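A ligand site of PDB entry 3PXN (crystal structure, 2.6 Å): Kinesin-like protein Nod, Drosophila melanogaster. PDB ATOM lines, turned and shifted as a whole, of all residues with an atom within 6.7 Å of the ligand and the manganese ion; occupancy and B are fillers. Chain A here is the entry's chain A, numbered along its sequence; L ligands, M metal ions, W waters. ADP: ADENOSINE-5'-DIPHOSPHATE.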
ATOM      1  N   ARG A  29       6.527   8.478  32.165  1.00  0.00           N
ATOM      2  CA  ARG A  29       5.921   9.702  31.679  1.00  0.00           C
ATOM      3  C   ARG A  29       4.468   9.409  31.305  1.00  0.00           C
ATOM      4  O   ARG A  29       4.165   8.428  30.604  1.00  0.00           O
ATOM      5  CB  ARG A  29       6.676  10.231  30.460  1.00  0.00           C
ATOM      6  CG  ARG A  29       6.133  11.594  29.981  1.00  0.00           C
ATOM      7  CD  ARG A  29       6.802  12.091  28.697  1.00  0.00           C
ATOM      8  NE  ARG A  29       6.627  13.528  28.531  1.00  0.00           N
ATOM      9  CZ  ARG A  29       7.070  14.230  27.508  1.00  0.00           C
ATOM     10  NH1 ARG A  29       7.724  13.627  26.521  1.00  0.00           N
ATOM     11  NH2 ARG A  29       6.874  15.536  27.438  1.00  0.00           N
ATOM     12  N   GLU A  30       3.568  10.253  31.784  1.00  0.00           N
ATOM     13  CA  GLU A  30       2.145  10.102  31.506  1.00  0.00           C
ATOM     14  C   GLU A  30       1.833  10.844  30.217  1.00  0.00           C
ATOM     15  O   GLU A  30       2.363  11.930  29.945  1.00  0.00           O
ATOM     16  CB  GLU A  30       1.328  10.673  32.658  1.00  0.00           C
ATOM     17  CG  GLU A  30      -0.161  10.709  32.417  1.00  0.00           C
ATOM     18  CD  GLU A  30      -0.884  11.524  33.470  1.00  0.00           C
ATOM     19  OE1 GLU A  30      -0.325  12.574  33.871  1.00  0.00           O
ATOM     20  OE2 GLU A  30      -1.978  11.105  33.905  1.00  0.00           O
ATOM     21  N   ALA A  31       0.986  10.211  29.413  1.00  0.00           N
ATOM     22  CA  ALA A  31       0.564  10.754  28.123  1.00  0.00           C
ATOM     23  C   ALA A  31      -0.616  11.676  28.329  1.00  0.00           C
ATOM     24  O   ALA A  31      -1.327  11.597  29.342  1.00  0.00           O
ATOM     25  CB  ALA A  31       0.178   9.613  27.188  1.00  0.00           C
ATOM     26  N   PRO A  32      -0.858  12.590  27.375  1.00  0.00           N
ATOM     27  CA  PRO A  32      -1.975  13.547  27.459  1.00  0.00           C
ATOM     28  C   PRO A  32      -3.322  12.836  27.614  1.00  0.00           C
ATOM     29  O   PRO A  32      -3.550  11.790  27.010  1.00  0.00           O
ATOM     30  CB  PRO A  32      -1.886  14.300  26.141  1.00  0.00           C
ATOM     31  CG  PRO A  32      -0.429  14.288  25.854  1.00  0.00           C
ATOM     32  CD  PRO A  32      -0.029  12.866  26.181  1.00  0.00           C
ATOM     33  N   ALA A  71       1.699  14.297  32.727  1.00  0.00           N
ATOM     34  CA  ALA A  71       1.382  14.799  31.392  1.00  0.00           C
ATOM     35  C   ALA A  71       1.705  16.276  31.174  1.00  0.00           C
ATOM     36  O   ALA A  71       1.860  16.693  30.036  1.00  0.00           O
ATOM     37  CB  ALA A  71      -0.089  14.532  31.081  1.00  0.00           C
ATOM     38  N   ILE A  73       4.474  17.899  31.928  1.00  0.00           N
ATOM     39  CA  ILE A  73       5.900  18.156  31.764  1.00  0.00           C
ATOM     40  C   ILE A  73       6.307  18.300  30.319  1.00  0.00           C
ATOM     41  O   ILE A  73       5.991  17.465  29.487  1.00  0.00           O
ATOM     42  CB  ILE A  73       6.737  17.038  32.408  1.00  0.00           C
ATOM     43  CG1 ILE A  73       6.331  16.913  33.870  1.00  0.00           C
ATOM     44  CG2 ILE A  73       8.237  17.361  32.290  1.00  0.00           C
ATOM     45  CD1 ILE A  73       6.584  18.157  34.674  1.00  0.00           C
ATOM     46  N   GLN A  75       8.887  18.783  26.901  1.00  0.00           N
ATOM     47  CA  GLN A  75      10.006  18.066  26.313  1.00  0.00           C
ATOM     48  C   GLN A  75      11.299  18.570  26.932  1.00  0.00           C
ATOM     49  O   GLN A  75      12.128  17.794  27.393  1.00  0.00           O
ATOM     50  CB  GLN A  75      10.038  18.313  24.804  1.00  0.00           C
ATOM     51  CG  GLN A  75       8.813  17.790  24.045  1.00  0.00           C
ATOM     52  CD  GLN A  75       8.889  16.307  23.762  1.00  0.00           C
ATOM     53  OE1 GLN A  75       8.889  15.483  24.666  1.00  0.00           O
ATOM     54  NE2 GLN A  75       8.951  15.957  22.478  1.00  0.00           N
ATOM     55  N   GLY A 102       6.450   0.744  26.001  1.00  0.00           N
ATOM     56  CA  GLY A 102       5.100   0.977  26.465  1.00  0.00           C
ATOM     57  C   GLY A 102       4.023   0.806  25.414  1.00  0.00           C
ATOM     58  O   GLY A 102       4.304   0.556  24.245  1.00  0.00           O
ATOM     59  N   GLN A 103       2.771   0.977  25.837  1.00  0.00           N
ATOM     60  CA  GLN A 103       1.630   0.831  24.938  1.00  0.00           C
ATOM     61  C   GLN A 103       1.711   1.816  23.761  1.00  0.00           C
ATOM     62  O   GLN A 103       2.215   2.922  23.889  1.00  0.00           O
ATOM     63  CB  GLN A 103       0.344   1.047  25.728  1.00  0.00           C
ATOM     64  CG  GLN A 103      -0.922   0.637  25.011  1.00  0.00           C
ATOM     65  CD  GLN A 103      -2.171   1.107  25.732  1.00  0.00           C
ATOM     66  OE1 GLN A 103      -3.274   0.649  25.436  1.00  0.00           O
ATOM     67  NE2 GLN A 103      -2.005   2.020  26.680  1.00  0.00           N
ATOM     68  N   THR A 104       1.174   1.395  22.623  1.00  0.00           N
ATOM     69  CA  THR A 104       1.178   2.236  21.438  1.00  0.00           C
ATOM     70  C   THR A 104       0.352   3.489  21.673  1.00  0.00           C
ATOM     71  O   THR A 104      -0.732   3.418  22.252  1.00  0.00           O
ATOM     72  CB  THR A 104       0.600   1.452  20.228  1.00  0.00           C
ATOM     73  OG1 THR A 104       1.480   0.366  19.915  1.00  0.00           O
ATOM     74  CG2 THR A 104       0.420   2.344  19.027  1.00  0.00           C
ATOM     75  N   GLY A 105       0.865   4.629  21.240  1.00  0.00           N
ATOM     76  CA  GLY A 105       0.135   5.867  21.438  1.00  0.00           C
ATOM     77  C   GLY A 105       0.372   6.572  22.765  1.00  0.00           C
ATOM     78  O   GLY A 105      -0.362   7.481  23.120  1.00  0.00           O
ATOM     79  N   THR A 106       1.410   6.170  23.495  1.00  0.00           N
ATOM     80  CA  THR A 106       1.706   6.776  24.783  1.00  0.00           C
ATOM     81  C   THR A 106       2.778   7.874  24.732  1.00  0.00           C
ATOM     82  O   THR A 106       3.193   8.385  25.765  1.00  0.00           O
ATOM     83  CB  THR A 106       2.111   5.676  25.818  1.00  0.00           C
ATOM     84  OG1 THR A 106       3.171   4.869  25.292  1.00  0.00           O
ATOM     85  CG2 THR A 106       0.912   4.801  26.136  1.00  0.00           C
ATOM     86  N   GLY A 107       3.213   8.225  23.531  1.00  0.00           N
ATOM     87  CA  GLY A 107       4.195   9.283  23.371  1.00  0.00           C
ATOM     88  C   GLY A 107       5.638   8.842  23.283  1.00  0.00           C
ATOM     89  O   GLY A 107       6.552   9.620  23.514  1.00  0.00           O
ATOM     90  N   LYS A 108       5.865   7.589  22.933  1.00  0.00           N
ATOM     91  CA  LYS A 108       7.233   7.104  22.850  1.00  0.00           C
ATOM     92  C   LYS A 108       8.004   7.774  21.717  1.00  0.00           C
ATOM     93  O   LYS A 108       9.045   8.364  21.937  1.00  0.00           O
ATOM     94  CB  LYS A 108       7.255   5.599  22.661  1.00  0.00           C
ATOM     95  CG  LYS A 108       6.665   4.845  23.810  1.00  0.00           C
ATOM     96  CD  LYS A 108       6.641   3.365  23.529  1.00  0.00           C
ATOM     97  CE  LYS A 108       5.786   3.081  22.311  1.00  0.00           C
ATOM     98  NZ  LYS A 108       5.598   1.617  22.190  1.00  0.00           N
ATOM     99  N   SER A 109       7.492   7.686  20.496  1.00  0.00           N
ATOM    100  CA  SER A 109       8.189   8.308  19.377  1.00  0.00           C
ATOM    101  C   SER A 109       8.313   9.806  19.536  1.00  0.00           C
ATOM    102  O   SER A 109       9.326  10.406  19.180  1.00  0.00           O
ATOM    103  CB  SER A 109       7.504   7.971  18.081  1.00  0.00           C
ATOM    104  OG  SER A 109       7.977   6.727  17.623  1.00  0.00           O
ATOM    105  N   TYR A 110       7.269  10.400  20.097  1.00  0.00           N
ATOM    106  CA  TYR A 110       7.236  11.828  20.335  1.00  0.00           C
ATOM    107  C   TYR A 110       8.328  12.191  21.332  1.00  0.00           C
ATOM    108  O   TYR A 110       9.062  13.167  21.129  1.00  0.00           O
ATOM    109  CB  TYR A 110       5.876  12.192  20.928  1.00  0.00           C
ATOM    110  CG  TYR A 110       5.776  13.609  21.456  1.00  0.00           C
ATOM    111  CD1 TYR A 110       5.521  14.682  20.576  1.00  0.00           C
ATOM    112  CD2 TYR A 110       5.934  13.886  22.810  1.00  0.00           C
ATOM    113  CE1 TYR A 110       5.404  15.983  21.057  1.00  0.00           C
ATOM    114  CE2 TYR A 110       5.831  15.188  23.300  1.00  0.00           C
ATOM    115  CZ  TYR A 110       5.559  16.227  22.411  1.00  0.00           C
ATOM    116  OH  TYR A 110       5.469  17.512  22.894  1.00  0.00           O
ATOM    117  N   SER A 111       8.414  11.417  22.402  1.00  0.00           N
ATOM    118  CA  SER A 111       9.398  11.636  23.447  1.00  0.00           C
ATOM    119  C   SER A 111      10.837  11.513  22.967  1.00  0.00           C
ATOM    120  O   SER A 111      11.658  12.358  23.293  1.00  0.00           O
ATOM    121  CB  SER A 111       9.164  10.663  24.613  1.00  0.00           C
ATOM    122  OG  SER A 111       7.950  10.992  25.274  1.00  0.00           O
ATOM    123  N   MET A 114      11.665  10.999  17.199  1.00  0.00           N
ATOM    124  CA  MET A 114      11.944  10.147  16.044  1.00  0.00           C
ATOM    125  C   MET A 114      11.350  10.688  14.740  1.00  0.00           C
ATOM    126  O   MET A 114      11.416  10.030  13.693  1.00  0.00           O
ATOM    127  CB  MET A 114      11.396   8.732  16.284  1.00  0.00           C
ATOM    128  CG  MET A 114      12.012   8.006  17.461  1.00  0.00           C
ATOM    129  SD  MET A 114      13.744   7.600  17.217  1.00  0.00           S
ATOM    130  CE  MET A 114      13.651   6.496  15.733  1.00  0.00           C
ATOM    131  N   HIS A 124       8.087  20.983  20.800  1.00  0.00           N
ATOM    132  CA  HIS A 124       7.789  19.551  20.680  1.00  0.00           C
ATOM    133  C   HIS A 124       8.946  18.659  20.243  1.00  0.00           C
ATOM    134  O   HIS A 124       8.788  17.447  20.117  1.00  0.00           O
ATOM    135  CB  HIS A 124       6.593  19.353  19.738  1.00  0.00           C
ATOM    136  CG  HIS A 124       5.330  20.013  20.206  1.00  0.00           C
ATOM    137  ND1 HIS A 124       4.755  19.740  21.427  1.00  0.00           N
ATOM    138  CD2 HIS A 124       4.528  20.928  19.608  1.00  0.00           C
ATOM    139  CE1 HIS A 124       3.657  20.453  21.566  1.00  0.00           C
ATOM    140  NE2 HIS A 124       3.491  21.181  20.479  1.00  0.00           N
ATOM    141  N   ARG A 206      11.415   2.480   6.079  1.00  0.00           N
ATOM    142  CA  ARG A 206      10.739   1.634   7.049  1.00  0.00           C
ATOM    143  C   ARG A 206       9.464   1.060   6.447  1.00  0.00           C
ATOM    144  O   ARG A 206       8.651   1.794   5.854  1.00  0.00           O
ATOM    145  CB  ARG A 206      10.395   2.435   8.300  1.00  0.00           C
ATOM    146  CG  ARG A 206      11.042   1.913   9.561  1.00  0.00           C
ATOM    147  CD  ARG A 206      10.730   2.838  10.723  1.00  0.00           C
ATOM    148  NE  ARG A 206      10.738   2.126  12.001  1.00  0.00           N
ATOM    149  CZ  ARG A 206      10.355   2.661  13.159  1.00  0.00           C
ATOM    150  NH1 ARG A 206       9.939   3.907  13.210  1.00  0.00           N
ATOM    151  NH2 ARG A 206      10.389   1.925  14.268  1.00  0.00           N
ATOM    152  N   SER A 220       7.696  -3.148  15.190  1.00  0.00           N
ATOM    153  CA  SER A 220       8.812  -2.428  14.587  1.00  0.00           C
ATOM    154  C   SER A 220       9.482  -1.496  15.592  1.00  0.00           C
ATOM    155  O   SER A 220       8.904  -0.479  15.977  1.00  0.00           O
ATOM    156  CB  SER A 220       8.320  -1.609  13.385  1.00  0.00           C
ATOM    157  OG  SER A 220       9.375  -0.847  12.823  1.00  0.00           O
ATOM    158  N   ASP A 241      13.499   3.345  20.450  1.00  0.00           N
ATOM    159  CA  ASP A 241      12.083   3.671  20.444  1.00  0.00           C
ATOM    160  C   ASP A 241      11.358   2.371  20.086  1.00  0.00           C
ATOM    161  O   ASP A 241      11.031   2.141  18.914  1.00  0.00           O
ATOM    162  CB  ASP A 241      11.867   4.767  19.409  1.00  0.00           C
ATOM    163  CG  ASP A 241      10.402   5.008  19.085  1.00  0.00           C
ATOM    164  OD1 ASP A 241      10.124   5.522  17.971  1.00  0.00           O
ATOM    165  OD2 ASP A 241       9.520   4.721  19.910  1.00  0.00           O
ATOM    166  N   LEU A 242      11.111   1.519  21.081  1.00  0.00           N
ATOM    167  CA  LEU A 242      10.465   0.224  20.853  1.00  0.00           C
ATOM    168  C   LEU A 242       9.036   0.371  20.388  1.00  0.00           C
ATOM    169  O   LEU A 242       8.424   1.425  20.576  1.00  0.00           O
ATOM    170  CB  LEU A 242      10.480  -0.630  22.137  1.00  0.00           C
ATOM    171  CG  LEU A 242      11.835  -1.012  22.713  1.00  0.00           C
ATOM    172  CD1 LEU A 242      11.656  -2.011  23.833  1.00  0.00           C
ATOM    173  CD2 LEU A 242      12.725  -1.577  21.618  1.00  0.00           C
ATOM    174  N   ALA A 243       8.500  -0.696  19.799  1.00  0.00           N
ATOM    175  CA  ALA A 243       7.127  -0.686  19.305  1.00  0.00           C
ATOM    176  C   ALA A 243       6.149  -1.029  20.428  1.00  0.00           C
ATOM    177  O   ALA A 243       6.573  -1.342  21.550  1.00  0.00           O
ATOM    178  CB  ALA A 243       6.986  -1.687  18.166  1.00  0.00           C
ATOM    179  N   GLY A 244       4.859  -0.962  20.123  1.00  0.00           N
ATOM    180  CA  GLY A 244       3.860  -1.283  21.119  1.00  0.00           C
ATOM    181  C   GLY A 244       4.257  -2.461  21.992  1.00  0.00           C
ATOM    182  O   GLY A 244       4.874  -3.416  21.518  1.00  0.00           O
ATOM    183  N   CYS A 311       6.411   4.884  28.991  1.00  0.00           N
ATOM    184  CA  CYS A 311       5.344   5.798  28.632  1.00  0.00           C
ATOM    185  C   CYS A 311       4.053   5.074  28.946  1.00  0.00           C
ATOM    186  O   CYS A 311       3.920   3.877  28.674  1.00  0.00           O
ATOM    187  CB  CYS A 311       5.412   6.132  27.158  1.00  0.00           C
ATOM    188  SG  CYS A 311       6.983   6.750  26.717  1.00  0.00           S
HETATM  189  PB  ADP L   1       3.768   6.054  20.148  1.00  0.00           P
HETATM  190  O1B ADP L   1       4.156   5.521  21.465  1.00  0.00           O
HETATM  191  O2B ADP L   1       5.078   6.448  19.322  1.00  0.00           O
HETATM  192  O3B ADP L   1       2.956   4.822  19.324  1.00  0.00           O
HETATM  193  PA  ADP L   1       3.356   8.689  19.670  1.00  0.00           P
HETATM  194  O1A ADP L   1       4.681   9.022  20.219  1.00  0.00           O
HETATM  195  O2A ADP L   1       3.462   8.440  18.064  1.00  0.00           O
HETATM  196  O3A ADP L   1       2.802   7.321  20.381  1.00  0.00           O
HETATM  197  O5' ADP L   1       2.358   9.853  19.999  1.00  0.00           O
HETATM  198  C5' ADP L   1       1.079   9.561  19.427  1.00  0.00           C
HETATM  199  C4' ADP L   1       0.420  10.885  19.180  1.00  0.00           C
HETATM  200  O4' ADP L   1       0.258  11.574  20.460  1.00  0.00           O
HETATM  201  C3' ADP L   1       1.286  11.788  18.241  1.00  0.00           C
HETATM  202  O3' ADP L   1       0.532  12.759  17.561  1.00  0.00           O
HETATM  203  C2' ADP L   1       2.024  12.631  19.359  1.00  0.00           C
HETATM  204  O2' ADP L   1       2.386  13.943  18.871  1.00  0.00           O
HETATM  205  C1' ADP L   1       0.935  12.853  20.436  1.00  0.00           C
HETATM  206  N9  ADP L   1       1.551  13.088  21.727  1.00  0.00           N
HETATM  207  C8  ADP L   1       2.086  12.097  22.551  1.00  0.00           C
HETATM  208  N7  ADP L   1       2.689  12.626  23.591  1.00  0.00           N
HETATM  209  C5  ADP L   1       2.432  13.954  23.598  1.00  0.00           C
HETATM  210  C6  ADP L   1       2.790  15.027  24.451  1.00  0.00           C
HETATM  211  N6  ADP L   1       3.452  14.782  25.643  1.00  0.00           N
HETATM  212  N1  ADP L   1       2.477  16.293  24.074  1.00  0.00           N
HETATM  213  C2  ADP L   1       1.727  16.529  22.994  1.00  0.00           C
HETATM  214  N3  ADP L   1       1.382  15.545  22.169  1.00  0.00           N
HETATM  215  C4  ADP L   1       1.726  14.282  22.396  1.00  0.00           C
HETATM  216 MN    MN M   1       6.072   5.032  17.853  1.00  0.00          MN
HETATM  217  O   HOH W   1       0.981   6.158  18.048  1.00  0.00           O
HETATM  218  O   HOH W   2       3.880   1.674  19.928  1.00  0.00           O
HETATM  219  O   HOH W   3       1.001  16.047  19.011  1.00  0.00           O
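The side-chain hydroxyl (OG) of Ser 109 lies close to the side-chain carboxylate (OD1) of Asp 241 (2.5 Å). The backbone carbonyl oxygen (O) of Ser 109 lies within hydrogen-bond range of the backbone NH (N) of Met 114 (3.1 Å). A ring nitrogen (ND1) of His 124 lies within hydrogen-bond range of the side-chain hydroxyl of Tyr 110 (2.8 Å). O of Tyr 110 lies within hydrogen-bond range of NE2 of Gln 75 (3.1 Å). The side-chain amino group of Lys 108 lies within hydrogen-bond range of the backbone carbonyl oxygen of Ala 243 (3.2 Å). The side-chain hydroxyl (OG) of Ser 111 is in hydrogen-bond range of the backbone carbonyl oxygen (O) of Gly 107, 2.6 Å away. NH2 of Arg 29 is in hydrogen-bond range of O of Ile 73 (2.9 Å). The side-chain amide oxygen (OE1) of Gln 75 lies within hydrogen-bond range of the guanidinium group (NH1) of Arg 29 (2.9 Å).
Arg 29 touches the ligand (NH2 to N6, 3.9 Å). CG of Pro 32 touches C6 of the ligand (3.6 Å). Thr 104 touches the ligand. Hydrophobic or aromatic side chains within 4 Å of the ligand: Pro 32 and Tyr 110. Nine residues have an atom within 4 Å of the ligand: Arg 29, Pro 32, Thr 104, Gly 105, Thr 106, Gly 107, Lys 108, Ser 109 and Tyr 110.
Water W2 lies within hydrogen-bond range of OG1 of Thr 104 (2.7 Å), N of Gly 244 (2.8 Å), NZ of Lys 108 (2.8 Å) and O3B of the ligand (3.3 Å).
One residue has an atom within 4 Å of the manganese ion: Ser 109. The nearest printed residue that does not touch the manganese ion is Asp 241 (4.03 Å).
The manganese ion is bound by O2B of the ligand, at 2.3 Å. OG of Ser 109 is bound to the manganese ion, at 2.6 Å. The manganese ion has two donor atoms within binding distance.
The backbone NH of Ser 109 is in hydrogen-bond range of an oxygen (O1A) of the ligand, 3.1 Å away. N of Gly 105 lies within hydrogen-bond range of O3B of the ligand (2.8 Å). The backbone NH of Tyr 110 lies within hydrogen-bond range of an oxygen (O1A) of the ligand (2.9 Å). OH of Tyr 110 is in hydrogen-bond range of N1 of the ligand (3.4 Å). The backbone NH (N) of Lys 108 lies close to an oxygen (O1B) of the ligand (3.1 Å). N of Gly 107 lies within hydrogen-bond range of O3A of the ligand (3.3 Å). An oxygen (O1B) of the ligand is in hydrogen-bond range of the backbone NH of Thr 106 (3.5 Å).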
